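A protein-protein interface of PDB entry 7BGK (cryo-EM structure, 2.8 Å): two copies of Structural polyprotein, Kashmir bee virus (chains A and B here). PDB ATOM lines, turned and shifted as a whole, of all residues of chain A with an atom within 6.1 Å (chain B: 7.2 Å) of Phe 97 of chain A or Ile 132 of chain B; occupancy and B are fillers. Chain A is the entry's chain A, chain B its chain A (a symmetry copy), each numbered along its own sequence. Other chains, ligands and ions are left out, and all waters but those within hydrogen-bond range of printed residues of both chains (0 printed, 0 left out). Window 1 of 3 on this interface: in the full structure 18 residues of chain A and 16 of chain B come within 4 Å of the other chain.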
ATOM      1  N   THR A  48     -17.683  30.318  13.096  1.00  0.00           N
ATOM      2  CA  THR A  48     -18.634  30.592  12.031  1.00  0.00           C
ATOM      3  C   THR A  48     -18.085  31.627  11.062  1.00  0.00           C
ATOM      4  O   THR A  48     -17.495  32.632  11.468  1.00  0.00           O
ATOM      5  CB  THR A  48     -19.962  31.078  12.606  1.00  0.00           C
ATOM      6  OG1 THR A  48     -19.761  32.287  13.342  1.00  0.00           O
ATOM      7  CG2 THR A  48     -20.561  30.039  13.511  1.00  0.00           C
ATOM      8  N   LYS A  95     -18.496  22.503   9.102  1.00  0.00           N
ATOM      9  CA  LYS A  95     -19.714  22.064   9.763  1.00  0.00           C
ATOM     10  C   LYS A  95     -20.861  22.932   9.282  1.00  0.00           C
ATOM     11  O   LYS A  95     -20.741  24.159   9.241  1.00  0.00           O
ATOM     12  CB  LYS A  95     -19.598  22.144  11.281  1.00  0.00           C
ATOM     13  CG  LYS A  95     -18.612  21.191  11.890  1.00  0.00           C
ATOM     14  CD  LYS A  95     -18.965  20.890  13.318  1.00  0.00           C
ATOM     15  CE  LYS A  95     -17.813  20.292  14.079  1.00  0.00           C
ATOM     16  NZ  LYS A  95     -17.286  19.052  13.472  1.00  0.00           N
ATOM     17  N   PHE A  96     -21.964  22.291   8.919  1.00  0.00           N
ATOM     18  CA  PHE A  96     -23.152  22.958   8.402  1.00  0.00           C
ATOM     19  C   PHE A  96     -24.312  22.618   9.326  1.00  0.00           C
ATOM     20  O   PHE A  96     -24.858  21.514   9.268  1.00  0.00           O
ATOM     21  CB  PHE A  96     -23.442  22.537   6.968  1.00  0.00           C
ATOM     22  CG  PHE A  96     -22.258  22.615   6.055  1.00  0.00           C
ATOM     23  CD1 PHE A  96     -22.040  23.737   5.288  1.00  0.00           C
ATOM     24  CD2 PHE A  96     -21.375  21.560   5.944  1.00  0.00           C
ATOM     25  CE1 PHE A  96     -20.967  23.809   4.444  1.00  0.00           C
ATOM     26  CE2 PHE A  96     -20.301  21.631   5.100  1.00  0.00           C
ATOM     27  CZ  PHE A  96     -20.097  22.758   4.349  1.00  0.00           C
ATOM     28  N   PHE A  97     -24.680  23.564  10.182  1.00  0.00           N
ATOM     29  CA  PHE A  97     -25.821  23.407  11.067  1.00  0.00           C
ATOM     30  C   PHE A  97     -27.073  23.899  10.357  1.00  0.00           C
ATOM     31  O   PHE A  97     -27.110  25.028   9.864  1.00  0.00           O
ATOM     32  CB  PHE A  97     -25.618  24.181  12.365  1.00  0.00           C
ATOM     33  CG  PHE A  97     -24.334  23.877  13.067  1.00  0.00           C
ATOM     34  CD1 PHE A  97     -24.307  23.028  14.152  1.00  0.00           C
ATOM     35  CD2 PHE A  97     -23.157  24.467  12.668  1.00  0.00           C
ATOM     36  CE1 PHE A  97     -23.132  22.762  14.804  1.00  0.00           C
ATOM     37  CE2 PHE A  97     -21.984  24.199  13.316  1.00  0.00           C
ATOM     38  CZ  PHE A  97     -21.971  23.347  14.382  1.00  0.00           C
ATOM     39  N   ASN A  98     -28.094  23.050  10.313  1.00  0.00           N
ATOM     40  CA  ASN A  98     -29.314  23.370   9.587  1.00  0.00           C
ATOM     41  C   ASN A  98     -30.142  24.403  10.336  1.00  0.00           C
ATOM     42  O   ASN A  98     -30.360  24.286  11.545  1.00  0.00           O
ATOM     43  CB  ASN A  98     -30.135  22.105   9.368  1.00  0.00           C
ATOM     44  CG  ASN A  98     -31.191  22.273   8.309  1.00  0.00           C
ATOM     45  OD1 ASN A  98     -30.950  22.866   7.259  1.00  0.00           O
ATOM     46  ND2 ASN A  98     -32.374  21.744   8.576  1.00  0.00           N
ATOM     47  N   THR A  99     -30.604  25.418   9.606  1.00  0.00           N
ATOM     48  CA  THR A  99     -31.508  26.433  10.129  1.00  0.00           C
ATOM     49  C   THR A  99     -32.643  26.692   9.151  1.00  0.00           C
ATOM     50  O   THR A  99     -33.124  27.821   9.032  1.00  0.00           O
ATOM     51  CB  THR A  99     -30.762  27.729  10.436  1.00  0.00           C
ATOM     52  OG1 THR A  99     -30.349  28.361   9.222  1.00  0.00           O
ATOM     53  CG2 THR A  99     -29.549  27.459  11.283  1.00  0.00           C
ATOM     54  N   PRO A 139     -28.890  17.316  12.139  1.00  0.00           N
ATOM     55  CA  PRO A 139     -28.810  18.665  11.573  1.00  0.00           C
ATOM     56  C   PRO A 139     -27.402  19.222  11.431  1.00  0.00           C
ATOM     57  O   PRO A 139     -27.263  20.420  11.175  1.00  0.00           O
ATOM     58  CB  PRO A 139     -29.619  19.494  12.575  1.00  0.00           C
ATOM     59  CG  PRO A 139     -29.561  18.743  13.823  1.00  0.00           C
ATOM     60  CD  PRO A 139     -29.508  17.319  13.473  1.00  0.00           C
ATOM     61  N   VAL A 140     -26.360  18.410  11.586  1.00  0.00           N
ATOM     62  CA  VAL A 140     -24.986  18.868  11.446  1.00  0.00           C
ATOM     63  C   VAL A 140     -24.277  17.917  10.492  1.00  0.00           C
ATOM     64  O   VAL A 140     -24.325  16.696  10.678  1.00  0.00           O
ATOM     65  CB  VAL A 140     -24.260  18.921  12.803  1.00  0.00           C
ATOM     66  CG1 VAL A 140     -22.874  19.497  12.640  1.00  0.00           C
ATOM     67  CG2 VAL A 140     -25.067  19.697  13.821  1.00  0.00           C
ATOM     68  N   HIS A 141     -23.612  18.474   9.480  1.00  0.00           N
ATOM     69  CA  HIS A 141     -23.023  17.664   8.421  1.00  0.00           C
ATOM     70  C   HIS A 141     -21.677  17.074   8.837  1.00  0.00           C
ATOM     71  O   HIS A 141     -21.499  15.851   8.842  1.00  0.00           O
ATOM     72  CB  HIS A 141     -22.884  18.506   7.157  1.00  0.00           C
ATOM     73  CG  HIS A 141     -22.626  17.707   5.921  1.00  0.00           C
ATOM     74  ND1 HIS A 141     -23.479  16.720   5.484  1.00  0.00           N
ATOM     75  CD2 HIS A 141     -21.623  17.763   5.016  1.00  0.00           C
ATOM     76  CE1 HIS A 141     -23.006  16.193   4.370  1.00  0.00           C
ATOM     77  NE2 HIS A 141     -21.880  16.807   4.065  1.00  0.00           N
ATOM     78  N   TYR A 170     -21.377  21.333  -2.201  1.00  0.00           N
ATOM     79  CA  TYR A 170     -22.476  21.209  -1.255  1.00  0.00           C
ATOM     80  C   TYR A 170     -23.782  21.133  -2.023  1.00  0.00           C
ATOM     81  O   TYR A 170     -24.108  22.045  -2.788  1.00  0.00           O
ATOM     82  CB  TYR A 170     -22.487  22.387  -0.285  1.00  0.00           C
ATOM     83  CG  TYR A 170     -23.115  22.094   1.051  1.00  0.00           C
ATOM     84  CD1 TYR A 170     -22.650  21.066   1.850  1.00  0.00           C
ATOM     85  CD2 TYR A 170     -24.161  22.866   1.523  1.00  0.00           C
ATOM     86  CE1 TYR A 170     -23.217  20.810   3.069  1.00  0.00           C
ATOM     87  CE2 TYR A 170     -24.733  22.618   2.736  1.00  0.00           C
ATOM     88  CZ  TYR A 170     -24.260  21.594   3.509  1.00  0.00           C
ATOM     89  OH  TYR A 170     -24.842  21.357   4.727  1.00  0.00           O
ATOM     90  N   GLN A 177     -31.092  26.582   4.902  1.00  0.00           N
ATOM     91  CA  GLN A 177     -30.252  27.597   5.514  1.00  0.00           C
ATOM     92  C   GLN A 177     -29.279  26.911   6.462  1.00  0.00           C
ATOM     93  O   GLN A 177     -29.602  25.889   7.073  1.00  0.00           O
ATOM     94  CB  GLN A 177     -31.081  28.645   6.258  1.00  0.00           C
ATOM     95  CG  GLN A 177     -31.860  29.568   5.356  1.00  0.00           C
ATOM     96  CD  GLN A 177     -32.645  30.605   6.126  1.00  0.00           C
ATOM     97  OE1 GLN A 177     -32.648  30.611   7.356  1.00  0.00           O
ATOM     98  NE2 GLN A 177     -33.313  31.494   5.403  1.00  0.00           N
ATOM     99  N   GLN A 178     -28.082  27.476   6.577  1.00  0.00           N
ATOM    100  CA  GLN A 178     -26.996  26.825   7.294  1.00  0.00           C
ATOM    101  C   GLN A 178     -26.209  27.820   8.132  1.00  0.00           C
ATOM    102  O   GLN A 178     -25.956  28.946   7.697  1.00  0.00           O
ATOM    103  CB  GLN A 178     -26.041  26.136   6.310  1.00  0.00           C
ATOM    104  CG  GLN A 178     -26.486  24.795   5.770  1.00  0.00           C
ATOM    105  CD  GLN A 178     -27.409  24.898   4.583  1.00  0.00           C
ATOM    106  OE1 GLN A 178     -28.446  24.248   4.546  1.00  0.00           O
ATOM    107  NE2 GLN A 178     -27.051  25.724   3.613  1.00  0.00           N
ATOM    108  N   ILE A 179     -25.819  27.394   9.331  1.00  0.00           N
ATOM    109  CA  ILE A 179     -24.696  27.993  10.044  1.00  0.00           C
ATOM    110  C   ILE A 179     -23.442  27.281   9.560  1.00  0.00           C
ATOM    111  O   ILE A 179     -23.299  26.069   9.745  1.00  0.00           O
ATOM    112  CB  ILE A 179     -24.832  27.856  11.569  1.00  0.00           C
ATOM    113  CG1 ILE A 179     -26.220  28.248  12.083  1.00  0.00           C
ATOM    114  CG2 ILE A 179     -23.761  28.669  12.250  1.00  0.00           C
ATOM    115  CD1 ILE A 179     -26.470  29.672  12.067  1.00  0.00           C
ATOM    116  N   VAL A 180     -22.533  28.021   8.939  1.00  0.00           N
ATOM    117  CA  VAL A 180     -21.332  27.439   8.356  1.00  0.00           C
ATOM    118  C   VAL A 180     -20.160  27.754   9.273  1.00  0.00           C
ATOM    119  O   VAL A 180     -19.722  28.904   9.370  1.00  0.00           O
ATOM    120  CB  VAL A 180     -21.085  27.950   6.933  1.00  0.00           C
ATOM    121  CG1 VAL A 180     -19.904  27.244   6.321  1.00  0.00           C
ATOM    122  CG2 VAL A 180     -22.306  27.743   6.085  1.00  0.00           C
ATOM    123  N   ALA A 181     -19.660  26.730   9.950  1.00  0.00           N
ATOM    124  CA  ALA A 181     -18.446  26.806  10.742  1.00  0.00           C
ATOM    125  C   ALA A 181     -17.361  25.977  10.075  1.00  0.00           C
ATOM    126  O   ALA A 181     -17.629  24.886   9.566  1.00  0.00           O
ATOM    127  CB  ALA A 181     -18.685  26.304  12.163  1.00  0.00           C
ATOM    128  N   THR B 107     -37.471  24.295  11.868  1.00  0.00           N
ATOM    129  CA  THR B 107     -36.207  23.967  12.507  1.00  0.00           C
ATOM    130  C   THR B 107     -35.959  24.978  13.610  1.00  0.00           C
ATOM    131  O   THR B 107     -35.620  26.132  13.337  1.00  0.00           O
ATOM    132  CB  THR B 107     -35.073  23.967  11.489  1.00  0.00           C
ATOM    133  OG1 THR B 107     -35.351  23.003  10.465  1.00  0.00           O
ATOM    134  CG2 THR B 107     -33.765  23.613  12.141  1.00  0.00           C
ATOM    135  N   TYR B 109     -33.670  25.966  16.882  1.00  0.00           N
ATOM    136  CA  TYR B 109     -32.345  25.720  17.414  1.00  0.00           C
ATOM    137  C   TYR B 109     -32.043  26.746  18.489  1.00  0.00           C
ATOM    138  O   TYR B 109     -32.494  27.890  18.433  1.00  0.00           O
ATOM    139  CB  TYR B 109     -31.267  25.747  16.322  1.00  0.00           C
ATOM    140  CG  TYR B 109     -31.058  27.068  15.621  1.00  0.00           C
ATOM    141  CD1 TYR B 109     -31.666  27.334  14.406  1.00  0.00           C
ATOM    142  CD2 TYR B 109     -30.219  28.031  16.153  1.00  0.00           C
ATOM    143  CE1 TYR B 109     -31.465  28.525  13.762  1.00  0.00           C
ATOM    144  CE2 TYR B 109     -30.014  29.223  15.514  1.00  0.00           C
ATOM    145  CZ  TYR B 109     -30.636  29.466  14.317  1.00  0.00           C
ATOM    146  OH  TYR B 109     -30.433  30.662  13.672  1.00  0.00           O
ATOM    147  N   VAL B 110     -31.277  26.306  19.475  1.00  0.00           N
ATOM    148  CA  VAL B 110     -30.833  27.135  20.582  1.00  0.00           C
ATOM    149  C   VAL B 110     -29.327  27.283  20.489  1.00  0.00           C
ATOM    150  O   VAL B 110     -28.615  26.312  20.213  1.00  0.00           O
ATOM    151  CB  VAL B 110     -31.249  26.539  21.939  1.00  0.00           C
ATOM    152  CG1 VAL B 110     -30.813  27.433  23.041  1.00  0.00           C
ATOM    153  CG2 VAL B 110     -32.739  26.364  21.999  1.00  0.00           C
ATOM    154  N   ARG B 111     -28.841  28.494  20.720  1.00  0.00           N
ATOM    155  CA  ARG B 111     -27.425  28.789  20.608  1.00  0.00           C
ATOM    156  C   ARG B 111     -26.993  29.666  21.768  1.00  0.00           C
ATOM    157  O   ARG B 111     -27.744  30.537  22.212  1.00  0.00           O
ATOM    158  CB  ARG B 111     -27.108  29.472  19.282  1.00  0.00           C
ATOM    159  CG  ARG B 111     -25.738  29.182  18.769  1.00  0.00           C
ATOM    160  CD  ARG B 111     -25.579  29.648  17.358  1.00  0.00           C
ATOM    161  NE  ARG B 111     -24.188  29.962  17.074  1.00  0.00           N
ATOM    162  CZ  ARG B 111     -23.791  30.780  16.111  1.00  0.00           C
ATOM    163  NH1 ARG B 111     -24.674  31.368  15.325  1.00  0.00           N
ATOM    164  NH2 ARG B 111     -22.503  31.010  15.940  1.00  0.00           N
ATOM    165  N   SER B 112     -25.782  29.428  22.257  1.00  0.00           N
ATOM    166  CA  SER B 112     -25.255  30.121  23.419  1.00  0.00           C
ATOM    167  C   SER B 112     -23.841  30.601  23.142  1.00  0.00           C
ATOM    168  O   SER B 112     -23.047  29.893  22.519  1.00  0.00           O
ATOM    169  CB  SER B 112     -25.260  29.207  24.644  1.00  0.00           C
ATOM    170  OG  SER B 112     -25.007  29.927  25.830  1.00  0.00           O
ATOM    171  N   SER B 130     -19.094  28.733  21.125  1.00  0.00           N
ATOM    172  CA  SER B 130     -20.540  28.675  21.174  1.00  0.00           C
ATOM    173  C   SER B 130     -20.973  27.232  21.373  1.00  0.00           C
ATOM    174  O   SER B 130     -20.171  26.300  21.305  1.00  0.00           O
ATOM    175  CB  SER B 130     -21.160  29.239  19.895  1.00  0.00           C
ATOM    176  OG  SER B 130     -22.567  29.308  20.001  1.00  0.00           O
ATOM    177  N   HIS B 131     -22.267  27.058  21.619  1.00  0.00           N
ATOM    178  CA  HIS B 131     -22.865  25.738  21.691  1.00  0.00           C
ATOM    179  C   HIS B 131     -24.273  25.823  21.135  1.00  0.00           C
ATOM    180  O   HIS B 131     -25.028  26.729  21.496  1.00  0.00           O
ATOM    181  CB  HIS B 131     -22.887  25.209  23.121  1.00  0.00           C
ATOM    182  CG  HIS B 131     -23.540  23.872  23.252  1.00  0.00           C
ATOM    183  ND1 HIS B 131     -23.379  22.873  22.319  1.00  0.00           N
ATOM    184  CD2 HIS B 131     -24.359  23.371  24.203  1.00  0.00           C
ATOM    185  CE1 HIS B 131     -24.072  21.814  22.690  1.00  0.00           C
ATOM    186  NE2 HIS B 131     -24.677  22.091  23.830  1.00  0.00           N
ATOM    187  N   ILE B 132     -24.618  24.888  20.261  1.00  0.00           N
ATOM    188  CA  ILE B 132     -25.900  24.878  19.575  1.00  0.00           C
ATOM    189  C   ILE B 132     -26.597  23.553  19.838  1.00  0.00           C
ATOM    190  O   ILE B 132     -25.972  22.489  19.790  1.00  0.00           O
ATOM    191  CB  ILE B 132     -25.727  25.124  18.064  1.00  0.00           C
ATOM    192  CG1 ILE B 132     -27.082  25.298  17.397  1.00  0.00           C
ATOM    193  CG2 ILE B 132     -24.985  23.989  17.415  1.00  0.00           C
ATOM    194  CD1 ILE B 132     -27.004  25.937  16.069  1.00  0.00           C
ATOM    195  N   THR B 133     -27.895  23.624  20.123  1.00  0.00           N
ATOM    196  CA  THR B 133     -28.728  22.452  20.320  1.00  0.00           C
ATOM    197  C   THR B 133     -30.019  22.615  19.536  1.00  0.00           C
ATOM    198  O   THR B 133     -30.401  23.718  19.146  1.00  0.00           O
ATOM    199  CB  THR B 133     -29.061  22.206  21.794  1.00  0.00           C
ATOM    200  OG1 THR B 133     -29.659  23.375  22.361  1.00  0.00           O
ATOM    201  CG2 THR B 133     -27.827  21.848  22.552  1.00  0.00           C
ATOM    202  N   TYR B 134     -30.683  21.490  19.312  1.00  0.00           N
ATOM    203  CA  TYR B 134     -31.963  21.461  18.615  1.00  0.00           C
ATOM    204  C   TYR B 134     -33.022  20.889  19.541  1.00  0.00           C
ATOM    205  O   TYR B 134     -33.041  19.665  19.775  1.00  0.00           O
ATOM    206  CB  TYR B 134     -31.850  20.643  17.333  1.00  0.00           C
ATOM    207  CG  TYR B 134     -31.108  21.377  16.249  1.00  0.00           C
ATOM    208  CD1 TYR B 134     -31.788  22.041  15.247  1.00  0.00           C
ATOM    209  CD2 TYR B 134     -29.727  21.431  16.244  1.00  0.00           C
ATOM    210  CE1 TYR B 134     -31.114  22.720  14.264  1.00  0.00           C
ATOM    211  CE2 TYR B 134     -29.048  22.108  15.269  1.00  0.00           C
ATOM    212  CZ  TYR B 134     -29.744  22.751  14.284  1.00  0.00           C
ATOM    213  OH  TYR B 134     -29.053  23.424  13.318  1.00  0.00           O
ATOM    214  N   ASN B 138     -32.788  17.334  21.030  1.00  0.00           N
ATOM    215  CA  ASN B 138     -32.188  17.537  22.348  1.00  0.00           C
ATOM    216  C   ASN B 138     -32.827  18.737  23.028  1.00  0.00           C
ATOM    217  O   ASN B 138     -32.388  19.878  22.838  1.00  0.00           O
ATOM    218  CB  ASN B 138     -30.681  17.727  22.246  1.00  0.00           C
ATOM    219  CG  ASN B 138     -30.011  17.762  23.592  1.00  0.00           C
ATOM    220  OD1 ASN B 138     -30.481  17.150  24.548  1.00  0.00           O
ATOM    221  ND2 ASN B 138     -28.910  18.484  23.679  1.00  0.00           N
ATOM    222  N   HIS B 141     -30.019  22.049  26.847  1.00  0.00           N
ATOM    223  CA  HIS B 141     -28.860  22.706  26.255  1.00  0.00           C
ATOM    224  C   HIS B 141     -27.554  22.243  26.897  1.00  0.00           C
ATOM    225  O   HIS B 141     -26.667  21.720  26.214  1.00  0.00           O
ATOM    226  CB  HIS B 141     -29.021  24.218  26.370  1.00  0.00           C
ATOM    227  CG  HIS B 141     -28.085  24.995  25.500  1.00  0.00           C
ATOM    228  ND1 HIS B 141     -28.041  24.841  24.134  1.00  0.00           N
ATOM    229  CD2 HIS B 141     -27.175  25.949  25.800  1.00  0.00           C
ATOM    230  CE1 HIS B 141     -27.134  25.656  23.631  1.00  0.00           C
ATOM    231  NE2 HIS B 141     -26.593  26.339  24.620  1.00  0.00           N
ATOM    232  N   VAL B 143     -24.972  23.982  28.585  1.00  0.00           N
ATOM    233  CA  VAL B 143     -23.774  24.775  28.353  1.00  0.00           C
ATOM    234  C   VAL B 143     -23.065  25.037  29.680  1.00  0.00           C
ATOM    235  O   VAL B 143     -23.655  24.958  30.758  1.00  0.00           O
ATOM    236  CB  VAL B 143     -24.115  26.091  27.633  1.00  0.00           C
ATOM    237  CG1 VAL B 143     -24.735  27.079  28.584  1.00  0.00           C
ATOM    238  CG2 VAL B 143     -22.889  26.672  26.987  1.00  0.00           C
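1 position is printed for both chains.
Of the 7 pairs that touch across the chains among the printed residues, none has its exchanged pair printed and touching as well.
Among the printed residues, pairs that only touch across the chains: Thr 48 of chain A with Arg 111 of chain B (3.3 Å), Thr 99 of chain A with Tyr 109 of chain B (3.3 Å), Phe 97 of chain A with Ile 132 of chain B (3.4 Å), Asn 98 of chain A with Thr 107 of chain B (3.5 Å), Phe 97 of chain A with Tyr 134 of chain B (3.6 Å) and Pro 139 of chain A with Tyr 134 of chain B (3.6 Å).
The backbone carbonyl oxygen (O) of Gln 177 of chain A sits close to the side-chain amide oxygen (OD1) of Asn 98 of chain A (3.3 Å).
O of Phe 97 of chain A sits at hydrogen-bond distance from N of Ile 179 of chain A (2.7 Å).
The backbone NH (N) of Thr 99 of chain A sits at hydrogen-bond distance from the backbone carbonyl oxygen (O) of Gln 177 of chain A, 2.8 Å away.
The guanidinium group (NE) of Arg 111 of chain B lies close to the side-chain hydroxyl (OG) of Ser 130 of chain B (3.4 Å).
The backbone NH (N) of Asn 98 of chain A is in hydrogen-bond range of the backbone carbonyl oxygen (O) of Pro 139 of chain A (2.9 Å).
Of the 13 printed residues of chain B, 5 touch a printed residue of chain A.
Printed residues of chain B that touch a printed residue of chain A: Thr 107, Tyr 109, Arg 111, Ile 132 and Tyr 134.
Hydrophobic or aromatic side chains of chain A that line the printed part of chain B: Phe 97 and Pro 139.
Among the printed residues, 7 pairs touch across the chains.
The backbone NH (N) of Asn 98 of chain A lies within hydrogen-bond range of the side-chain hydroxyl (OH) of Tyr 134 of chain B.
Printed residues of chain B within 4 Å of Thr 48 of chain A: Arg 111 (3.3 Å).
Phe 96 of chain A touches none of the printed residues of chain B.
Phe 97 of chain A touches just these residues of chain B: Ile 132 and Tyr 134.
Of the printed residues of chain B, Asn 98 of chain A touches Thr 107 and Tyr 134.
Printed residues of chain B within 4 Å of Pro 139 of chain A: Tyr 134.
Ile 132 of chain B touches just one residue of chain A: Phe 97 (3.4 Å).
Asn 138 of chain B touches none of the printed residues of chain A.
The nearest residue of chain B that does not touch Phe 97 of chain A is Tyr 109 of chain B (6.8 Å).
The nearest residue of chain A that does not touch Ile 132 of chain B is Ile 179 of chain A (4.7 Å).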
